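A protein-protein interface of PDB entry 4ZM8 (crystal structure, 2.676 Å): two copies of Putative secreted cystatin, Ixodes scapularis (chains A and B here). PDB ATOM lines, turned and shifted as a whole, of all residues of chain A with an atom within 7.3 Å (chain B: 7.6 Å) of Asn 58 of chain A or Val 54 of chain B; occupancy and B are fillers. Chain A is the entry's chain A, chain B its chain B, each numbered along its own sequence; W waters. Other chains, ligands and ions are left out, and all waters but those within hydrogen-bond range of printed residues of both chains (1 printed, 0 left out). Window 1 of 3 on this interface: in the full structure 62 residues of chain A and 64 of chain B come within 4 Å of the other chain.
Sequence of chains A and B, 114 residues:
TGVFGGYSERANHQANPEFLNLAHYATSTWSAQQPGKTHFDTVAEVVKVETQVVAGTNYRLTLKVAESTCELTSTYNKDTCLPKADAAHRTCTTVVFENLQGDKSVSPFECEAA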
ATOM      1  N   VAL A  54      -0.848  19.876  16.894  1.00  0.00           N
ATOM      2  CA  VAL A  54      -0.930  18.571  17.545  1.00  0.00           C
ATOM      3  C   VAL A  54      -2.238  18.431  18.298  1.00  0.00           C
ATOM      4  O   VAL A  54      -2.508  19.196  19.223  1.00  0.00           O
ATOM      5  CB  VAL A  54       0.209  18.337  18.546  1.00  0.00           C
ATOM      6  CG1 VAL A  54      -0.008  17.022  19.259  1.00  0.00           C
ATOM      7  CG2 VAL A  54       1.567  18.357  17.849  1.00  0.00           C
ATOM      8  N   ALA A  55      -3.045  17.457  17.899  1.00  0.00           N
ATOM      9  CA  ALA A  55      -4.275  17.151  18.607  1.00  0.00           C
ATOM     10  C   ALA A  55      -4.417  15.656  18.810  1.00  0.00           C
ATOM     11  O   ALA A  55      -4.310  14.865  17.860  1.00  0.00           O
ATOM     12  CB  ALA A  55      -5.469  17.687  17.862  1.00  0.00           C
ATOM     13  N   GLY A  56      -4.662  15.275  20.058  1.00  0.00           N
ATOM     14  CA  GLY A  56      -4.942  13.897  20.389  1.00  0.00           C
ATOM     15  C   GLY A  56      -5.266  13.690  21.852  1.00  0.00           C
ATOM     16  O   GLY A  56      -5.439  14.645  22.597  1.00  0.00           O
ATOM     17  N   THR A  57      -5.341  12.422  22.246  1.00  0.00           N
ATOM     18  CA  THR A  57      -5.605  12.024  23.616  1.00  0.00           C
ATOM     19  C   THR A  57      -4.599  10.967  24.015  1.00  0.00           C
ATOM     20  O   THR A  57      -4.350  10.035  23.261  1.00  0.00           O
ATOM     21  CB  THR A  57      -7.030  11.465  23.773  1.00  0.00           C
ATOM     22  OG1 THR A  57      -7.984  12.456  23.361  1.00  0.00           O
ATOM     23  CG2 THR A  57      -7.300  11.020  25.216  1.00  0.00           C
ATOM     24  N   ASN A  58      -4.000  11.118  25.186  1.00  0.00           N
ATOM     25  CA  ASN A  58      -3.139  10.073  25.713  1.00  0.00           C
ATOM     26  C   ASN A  58      -3.943   9.126  26.602  1.00  0.00           C
ATOM     27  O   ASN A  58      -4.640   9.566  27.505  1.00  0.00           O
ATOM     28  CB  ASN A  58      -1.975  10.673  26.492  1.00  0.00           C
ATOM     29  CG  ASN A  58      -0.720  10.764  25.667  1.00  0.00           C
ATOM     30  OD1 ASN A  58      -0.587  10.081  24.664  1.00  0.00           O
ATOM     31  ND2 ASN A  58       0.213  11.587  26.093  1.00  0.00           N
ATOM     32  N   TYR A  59      -3.870   7.831  26.327  1.00  0.00           N
ATOM     33  CA  TYR A  59      -4.515   6.844  27.182  1.00  0.00           C
ATOM     34  C   TYR A  59      -3.469   6.046  27.952  1.00  0.00           C
ATOM     35  O   TYR A  59      -2.773   5.219  27.377  1.00  0.00           O
ATOM     36  CB  TYR A  59      -5.386   5.894  26.363  1.00  0.00           C
ATOM     37  CG  TYR A  59      -6.471   6.580  25.567  1.00  0.00           C
ATOM     38  CD1 TYR A  59      -6.183   7.222  24.365  1.00  0.00           C
ATOM     39  CD2 TYR A  59      -7.782   6.593  26.016  1.00  0.00           C
ATOM     40  CE1 TYR A  59      -7.172   7.844  23.639  1.00  0.00           C
ATOM     41  CE2 TYR A  59      -8.781   7.220  25.287  1.00  0.00           C
ATOM     42  CZ  TYR A  59      -8.468   7.843  24.104  1.00  0.00           C
ATOM     43  OH  TYR A  59      -9.458   8.469  23.388  1.00  0.00           O
ATOM     44  N   ARG A  60      -3.347   6.286  29.249  1.00  0.00           N
ATOM     45  CA  ARG A  60      -2.477   5.438  30.042  1.00  0.00           C
ATOM     46  C   ARG A  60      -3.262   4.219  30.523  1.00  0.00           C
ATOM     47  O   ARG A  60      -4.329   4.354  31.127  1.00  0.00           O
ATOM     48  CB  ARG A  60      -1.885   6.199  31.218  1.00  0.00           C
ATOM     49  CG  ARG A  60      -0.737   5.476  31.878  1.00  0.00           C
ATOM     50  CD  ARG A  60       0.165   6.462  32.593  1.00  0.00           C
ATOM     51  NE  ARG A  60      -0.553   7.220  33.614  1.00  0.00           N
ATOM     52  CZ  ARG A  60      -0.121   8.363  34.146  1.00  0.00           C
ATOM     53  NH1 ARG A  60       1.023   8.903  33.750  1.00  0.00           N
ATOM     54  NH2 ARG A  60      -0.850   8.974  35.066  1.00  0.00           N
ATOM     55  N   LEU A  61      -2.740   3.028  30.245  1.00  0.00           N
ATOM     56  CA  LEU A  61      -3.453   1.805  30.579  1.00  0.00           C
ATOM     57  C   LEU A  61      -2.733   0.951  31.612  1.00  0.00           C
ATOM     58  O   LEU A  61      -1.535   0.670  31.497  1.00  0.00           O
ATOM     59  CB  LEU A  61      -3.696   0.982  29.315  1.00  0.00           C
ATOM     60  CG  LEU A  61      -4.416   1.789  28.233  1.00  0.00           C
ATOM     61  CD1 LEU A  61      -4.773   0.925  27.045  1.00  0.00           C
ATOM     62  CD2 LEU A  61      -5.646   2.465  28.794  1.00  0.00           C
ATOM     63  N   VAL A  95       1.193   3.735  27.486  1.00  0.00           N
ATOM     64  CA  VAL A  95       0.424   4.870  27.008  1.00  0.00           C
ATOM     65  C   VAL A  95       0.129   4.689  25.535  1.00  0.00           C
ATOM     66  O   VAL A  95       0.975   4.227  24.779  1.00  0.00           O
ATOM     67  CB  VAL A  95       1.147   6.206  27.203  1.00  0.00           C
ATOM     68  CG1 VAL A  95       0.157   7.349  26.997  1.00  0.00           C
ATOM     69  CG2 VAL A  95       1.801   6.282  28.571  1.00  0.00           C
ATOM     70  N   VAL A  96      -1.081   5.058  25.139  1.00  0.00           N
ATOM     71  CA  VAL A  96      -1.504   4.984  23.762  1.00  0.00           C
ATOM     72  C   VAL A  96      -2.010   6.343  23.335  1.00  0.00           C
ATOM     73  O   VAL A  96      -3.079   6.786  23.767  1.00  0.00           O
ATOM     74  CB  VAL A  96      -2.624   3.937  23.544  1.00  0.00           C
ATOM     75  CG1 VAL A  96      -3.168   4.010  22.108  1.00  0.00           C
ATOM     76  CG2 VAL A  96      -2.134   2.541  23.871  1.00  0.00           C
ATOM     77  N   PHE A  97      -1.235   7.012  22.490  1.00  0.00           N
ATOM     78  CA  PHE A  97      -1.679   8.261  21.899  1.00  0.00           C
ATOM     79  C   PHE A  97      -2.549   7.991  20.681  1.00  0.00           C
ATOM     80  O   PHE A  97      -2.295   7.066  19.922  1.00  0.00           O
ATOM     81  CB  PHE A  97      -0.495   9.131  21.496  1.00  0.00           C
ATOM     82  CG  PHE A  97      -0.900  10.417  20.845  1.00  0.00           C
ATOM     83  CD1 PHE A  97      -1.300  11.489  21.608  1.00  0.00           C
ATOM     84  CD2 PHE A  97      -0.907  10.538  19.472  1.00  0.00           C
ATOM     85  CE1 PHE A  97      -1.688  12.668  21.018  1.00  0.00           C
ATOM     86  CE2 PHE A  97      -1.298  11.714  18.870  1.00  0.00           C
ATOM     87  CZ  PHE A  97      -1.684  12.787  19.647  1.00  0.00           C
ATOM     88  N   GLU A  98      -3.575   8.811  20.506  1.00  0.00           N
ATOM     89  CA  GLU A  98      -4.411   8.743  19.329  1.00  0.00           C
ATOM     90  C   GLU A  98      -4.683  10.153  18.808  1.00  0.00           C
ATOM     91  O   GLU A  98      -5.258  10.978  19.511  1.00  0.00           O
ATOM     92  CB  GLU A  98      -5.715   8.024  19.648  1.00  0.00           C
ATOM     93  CG  GLU A  98      -6.714   7.972  18.504  1.00  0.00           C
ATOM     94  CD  GLU A  98      -7.899   7.066  18.814  1.00  0.00           C
ATOM     95  OE1 GLU A  98      -8.544   7.261  19.865  1.00  0.00           O
ATOM     96  OE2 GLU A  98      -8.173   6.149  18.012  1.00  0.00           O
ATOM     97  N   SER A 105      -0.391   5.326  18.532  1.00  0.00           N
ATOM     98  CA  SER A 105       0.960   4.895  18.872  1.00  0.00           C
ATOM     99  C   SER A 105       0.948   4.230  20.238  1.00  0.00           C
ATOM    100  O   SER A 105       0.108   4.536  21.072  1.00  0.00           O
ATOM    101  CB  SER A 105       1.935   6.067  18.878  1.00  0.00           C
ATOM    102  OG  SER A 105       1.786   6.844  20.059  1.00  0.00           O
ATOM    103  N   GLY B   5      -3.616  19.523  33.094  1.00  0.00           N
ATOM    104  CA  GLY B   5      -2.632  19.192  32.083  1.00  0.00           C
ATOM    105  C   GLY B   5      -2.142  17.768  32.239  1.00  0.00           C
ATOM    106  O   GLY B   5      -1.412  17.255  31.395  1.00  0.00           O
ATOM    107  N   TYR B   7      -3.119  13.542  33.756  1.00  0.00           N
ATOM    108  CA  TYR B   7      -4.115  12.508  33.486  1.00  0.00           C
ATOM    109  C   TYR B   7      -5.331  12.631  34.408  1.00  0.00           C
ATOM    110  O   TYR B   7      -5.275  13.292  35.439  1.00  0.00           O
ATOM    111  CB  TYR B   7      -3.488  11.113  33.615  1.00  0.00           C
ATOM    112  CG  TYR B   7      -2.577  10.714  32.462  1.00  0.00           C
ATOM    113  CD1 TYR B   7      -3.096  10.138  31.315  1.00  0.00           C
ATOM    114  CD2 TYR B   7      -1.207  10.918  32.520  1.00  0.00           C
ATOM    115  CE1 TYR B   7      -2.282   9.772  30.263  1.00  0.00           C
ATOM    116  CE2 TYR B   7      -0.387  10.546  31.474  1.00  0.00           C
ATOM    117  CZ  TYR B   7      -0.934   9.976  30.345  1.00  0.00           C
ATOM    118  OH  TYR B   7      -0.136   9.604  29.288  1.00  0.00           O
ATOM    119  N   SER B   8      -6.435  12.008  34.007  1.00  0.00           N
ATOM    120  CA  SER B   8      -7.655  11.953  34.814  1.00  0.00           C
ATOM    121  C   SER B   8      -8.220  10.532  34.814  1.00  0.00           C
ATOM    122  O   SER B   8      -8.569  10.001  33.754  1.00  0.00           O
ATOM    123  CB  SER B   8      -8.702  12.931  34.283  1.00  0.00           C
ATOM    124  OG  SER B   8      -8.122  14.194  34.018  1.00  0.00           O
ATOM    125  N   LEU B  22      -9.169  -0.476  22.778  1.00  0.00           N
ATOM    126  CA  LEU B  22      -7.877   0.199  22.701  1.00  0.00           C
ATOM    127  C   LEU B  22      -6.775  -0.536  23.481  1.00  0.00           C
ATOM    128  O   LEU B  22      -5.581  -0.432  23.174  1.00  0.00           O
ATOM    129  CB  LEU B  22      -8.044   1.611  23.232  1.00  0.00           C
ATOM    130  CG  LEU B  22      -7.087   2.684  22.790  1.00  0.00           C
ATOM    131  CD1 LEU B  22      -6.781   2.473  21.327  1.00  0.00           C
ATOM    132  CD2 LEU B  22      -7.811   3.978  23.022  1.00  0.00           C
ATOM    133  N   VAL B  49      -7.666   3.095  33.687  1.00  0.00           N
ATOM    134  CA  VAL B  49      -7.588   3.942  32.504  1.00  0.00           C
ATOM    135  C   VAL B  49      -7.459   5.406  32.881  1.00  0.00           C
ATOM    136  O   VAL B  49      -8.177   5.892  33.751  1.00  0.00           O
ATOM    137  CB  VAL B  49      -8.813   3.781  31.618  1.00  0.00           C
ATOM    138  CG1 VAL B  49      -8.743   4.750  30.448  1.00  0.00           C
ATOM    139  CG2 VAL B  49      -8.895   2.353  31.123  1.00  0.00           C
ATOM    140  N   GLU B  50      -6.534   6.108  32.235  1.00  0.00           N
ATOM    141  CA  GLU B  50      -6.411   7.552  32.404  1.00  0.00           C
ATOM    142  C   GLU B  50      -6.274   8.237  31.041  1.00  0.00           C
ATOM    143  O   GLU B  50      -5.514   7.783  30.185  1.00  0.00           O
ATOM    144  CB  GLU B  50      -5.211   7.887  33.294  1.00  0.00           C
ATOM    145  CG  GLU B  50      -5.190   7.132  34.601  1.00  0.00           C
ATOM    146  CD  GLU B  50      -3.818   7.092  35.228  1.00  0.00           C
ATOM    147  OE1 GLU B  50      -3.037   6.182  34.882  1.00  0.00           O
ATOM    148  OE2 GLU B  50      -3.513   7.977  36.058  1.00  0.00           O
ATOM    149  N   THR B  51      -7.011   9.322  30.832  1.00  0.00           N
ATOM    150  CA  THR B  51      -6.828  10.104  29.624  1.00  0.00           C
ATOM    151  C   THR B  51      -6.223  11.452  29.940  1.00  0.00           C
ATOM    152  O   THR B  51      -6.340  11.958  31.052  1.00  0.00           O
ATOM    153  CB  THR B  51      -8.130  10.333  28.857  1.00  0.00           C
ATOM    154  OG1 THR B  51      -8.919  11.322  29.526  1.00  0.00           O
ATOM    155  CG2 THR B  51      -8.905   9.040  28.720  1.00  0.00           C
ATOM    156  N   GLN B  52      -5.572  12.011  28.927  1.00  0.00           N
ATOM    157  CA  GLN B  52      -4.883  13.287  28.990  1.00  0.00           C
ATOM    158  C   GLN B  52      -4.899  13.886  27.599  1.00  0.00           C
ATOM    159  O   GLN B  52      -4.402  13.275  26.643  1.00  0.00           O
ATOM    160  CB  GLN B  52      -3.450  13.117  29.464  1.00  0.00           C
ATOM    161  CG  GLN B  52      -2.593  14.350  29.250  1.00  0.00           C
ATOM    162  CD  GLN B  52      -1.117  14.030  29.286  1.00  0.00           C
ATOM    163  OE1 GLN B  52      -0.533  13.615  28.284  1.00  0.00           O
ATOM    164  NE2 GLN B  52      -0.510  14.190  30.453  1.00  0.00           N
ATOM    165  N   VAL B  53      -5.499  15.059  27.461  1.00  0.00           N
ATOM    166  CA  VAL B  53      -5.553  15.695  26.159  1.00  0.00           C
ATOM    167  C   VAL B  53      -4.179  16.242  25.817  1.00  0.00           C
ATOM    168  O   VAL B  53      -3.532  16.875  26.654  1.00  0.00           O
ATOM    169  CB  VAL B  53      -6.575  16.832  26.111  1.00  0.00           C
ATOM    170  CG1 VAL B  53      -6.512  17.539  24.754  1.00  0.00           C
ATOM    171  CG2 VAL B  53      -7.969  16.311  26.407  1.00  0.00           C
ATOM    172  N   VAL B  54      -3.727  15.972  24.599  1.00  0.00           N
ATOM    173  CA  VAL B  54      -2.476  16.524  24.117  1.00  0.00           C
ATOM    174  C   VAL B  54      -2.787  17.463  22.971  1.00  0.00           C
ATOM    175  O   VAL B  54      -3.200  17.026  21.900  1.00  0.00           O
ATOM    176  CB  VAL B  54      -1.497  15.438  23.657  1.00  0.00           C
ATOM    177  CG1 VAL B  54      -0.274  16.073  23.021  1.00  0.00           C
ATOM    178  CG2 VAL B  54      -1.078  14.571  24.836  1.00  0.00           C
ATOM    179  N   ALA B  55      -2.628  18.758  23.215  1.00  0.00           N
ATOM    180  CA  ALA B  55      -2.954  19.765  22.218  1.00  0.00           C
ATOM    181  C   ALA B  55      -1.935  20.874  22.267  1.00  0.00           C
ATOM    182  O   ALA B  55      -1.473  21.257  23.336  1.00  0.00           O
ATOM    183  CB  ALA B  55      -4.346  20.320  22.441  1.00  0.00           C
ATOM    184  N   GLY B  56      -1.591  21.395  21.101  1.00  0.00           N
ATOM    185  CA  GLY B  56      -0.601  22.440  21.010  1.00  0.00           C
ATOM    186  C   GLY B  56      -0.159  22.569  19.577  1.00  0.00           C
ATOM    187  O   GLY B  56      -0.916  22.247  18.646  1.00  0.00           O
ATOM    188  N   PHE B  97       7.936  22.024  20.981  1.00  0.00           N
ATOM    189  CA  PHE B  97       6.503  21.790  21.200  1.00  0.00           C
ATOM    190  C   PHE B  97       5.951  22.727  22.268  1.00  0.00           C
ATOM    191  O   PHE B  97       6.573  22.927  23.302  1.00  0.00           O
ATOM    192  CB  PHE B  97       6.210  20.337  21.606  1.00  0.00           C
ATOM    193  CG  PHE B  97       4.767  20.111  21.994  1.00  0.00           C
ATOM    194  CD1 PHE B  97       3.776  20.052  21.027  1.00  0.00           C
ATOM    195  CD2 PHE B  97       4.395  20.007  23.321  1.00  0.00           C
ATOM    196  CE1 PHE B  97       2.450  19.882  21.369  1.00  0.00           C
ATOM    197  CE2 PHE B  97       3.060  19.835  23.673  1.00  0.00           C
ATOM    198  CZ  PHE B  97       2.093  19.769  22.690  1.00  0.00           C
ATOM    199  N   ASN B  99       2.386  23.379  24.180  1.00  0.00           N
ATOM    200  CA  ASN B  99       0.996  23.165  24.526  1.00  0.00           C
ATOM    201  C   ASN B  99       0.418  24.466  25.057  1.00  0.00           C
ATOM    202  O   ASN B  99       1.154  25.424  25.281  1.00  0.00           O
ATOM    203  CB  ASN B  99       0.855  22.030  25.545  1.00  0.00           C
ATOM    204  CG  ASN B  99       1.679  22.254  26.794  1.00  0.00           C
ATOM    205  OD1 ASN B  99       1.763  23.367  27.310  1.00  0.00           O
ATOM    206  ND2 ASN B  99       2.298  21.188  27.287  1.00  0.00           N
ATOM    207  N   LEU B 100      -0.893  24.482  25.270  1.00  0.00           N
ATOM    208  CA  LEU B 100      -1.627  25.705  25.557  1.00  0.00           C
ATOM    209  C   LEU B 100      -1.091  26.402  26.804  1.00  0.00           C
ATOM    210  O   LEU B 100      -1.075  27.635  26.885  1.00  0.00           O
ATOM    211  CB  LEU B 100      -3.112  25.394  25.728  1.00  0.00           C
ATOM    212  CG  LEU B 100      -3.751  24.442  24.710  1.00  0.00           C
ATOM    213  CD1 LEU B 100      -5.248  24.367  24.916  1.00  0.00           C
ATOM    214  CD2 LEU B 100      -3.436  24.864  23.293  1.00  0.00           C
HETATM  215  O   HOH W   1      -3.810   3.748  33.705  1.00  0.00           O
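The backbone NH of Val 54 of chain A sits at hydrogen-bond distance from the backbone carbonyl oxygen of Gly 56 of chain B, 2.9 Å away. The backbone NH of Gly 56 of chain A is in hydrogen-bond range of the backbone carbonyl oxygen of Val 54 of chain B, 2.9 Å away. The backbone NH (N) of Asn 58 of chain A is in hydrogen-bond range of the backbone carbonyl oxygen (O) of Gln 52 of chain B (2.6 Å). The guanidinium group of Arg 60 of chain A is in salt-bridge range of the side-chain carboxylate of Glu 50 of chain B (3.0 Å). The backbone carbonyl oxygen of Glu 50 of chain B lies close to the backbone carbonyl oxygen of Asn 58 of chain A (3.3 Å).
The backbone NH (N) of Thr 57 of chain A lies within hydrogen-bond range of the backbone carbonyl oxygen (O) of Glu 98 of chain A, 3.1 Å away. O of Tyr 59 of chain A is in hydrogen-bond range of N of Val 96 of chain A. N of Ser 105 of chain A lies within hydrogen-bond range of O of Phe 97 of chain A, 2.9 Å away. O of Gly 5 of chain B lies within hydrogen-bond range of NE2 of Gln 52 of chain B (3.3 Å). The backbone NH of Ser 8 of chain B is in hydrogen-bond range of the backbone carbonyl oxygen of Thr 51 of chain B (3.0 Å).
Val 54 of chain A touches Val 54 of chain B. Val 54 of chain A touches Ala 55 of chain B. Thr 57 of chain A touches Thr 51 of chain B. ND2 of Asn 58 of chain A touches CG2 of Val 54 of chain B, at 3.5 Å. Leu 22 of chain B touches Tyr 59 of chain A (CD2 to CD1, 3.9 Å). Tyr 59 of chain A touches Glu 50 of chain B (CA to O, 3.3 Å). Tyr 59 of chain A touches Thr 51 of chain B. Tyr 7 of chain B touches Arg 60 of chain A (CE2 to NH1, 3.1 Å). Leu 61 of chain A touches Val 49 of chain B. Val 95 of chain A touches Tyr 7 of chain B (CG1 to OH, 3.2 Å).
Printed residues of chain B within 4 Å of Thr 57 of chain A: Thr 51 (3.8 Å) and Gln 52 (3.5 Å). Asn 58 of chain A touches five residues of chain B. Of the printed residues of chain B, Tyr 59 of chain A touches Leu 22, Glu 50 and Thr 51. Printed residues of chain B within 4 Å of Phe 97 of chain A: Val 54. Gly 5 of chain B touches none of the printed residues of chain A. Printed residues of chain A within 4 Å of Val 54 of chain B: Val 54 (3.5 Å), Ala 55 (3.5 Å), Gly 56 (2.9 Å), Asn 58 (3.5 Å) and Phe 97 (3.8 Å). Of the printed residues of chain A, Ala 55 of chain B touches Val 54. Of the printed residues of chain A, Phe 97 of chain B touches Val 54. Asn 99 of chain B touches none of the printed residues of chain A. The nearest residue of chain B that does not touch Asn 58 of chain A is Val 53 of chain B (4.8 Å). The nearest residue of chain A that does not touch Val 54 of chain B is Thr 57 of chain A (4.5 Å). The nearest printed residue of chain A that does not touch Val 53 of chain B is Thr 57 of chain A (4.5 Å).
Of the 13 printed residues of chain A, 10 touch a printed residue of chain B. Hydrophobic or aromatic side chains of chain A within 4 Å of the printed part of chain B: Val 54, Tyr 59, Leu 61, Val 95 and Phe 97. Hydrophobic or aromatic side chains of chain B within 4 Å of the printed part of chain A: Tyr 7, Leu 22, Val 49, Val 53, Val 54, Ala 55 and Phe 97. Among the printed residues, Asp or Glu carboxylates within 4 Å of a Lys or Arg side-chain nitrogen of the other chain: Arg 60 of chain A with Glu 50 of chain B (3.0 Å).
Val 54 of chain B touches its own counterpart, Val 54 of chain A. Val 54 of chain A touches Ala 55 of chain B, and with the chains exchanged Ala 55 of chain A touches Val 54 of chain B. Val 54 of chain A touches Gly 56 of chain B, and with the chains exchanged Gly 56 of chain A touches Val 54 of chain B. Val 54 of chain A touches Phe 97 of chain B, and with the chains exchanged Phe 97 of chain A touches Val 54 of chain B. Positions printed for both chains: 54, 55, 56 and 97. Of the 23 pairs that touch across the chains among the printed residues, 7 have their exchanged pair printed and touching as well.
Water W1 lies within hydrogen-bond range of the backbone carbonyl oxygen (O) of Arg 60 of chain A (2.7 Å) and the side-chain carboxylate (OE1) of Glu 50 of chain B (2.8 Å).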
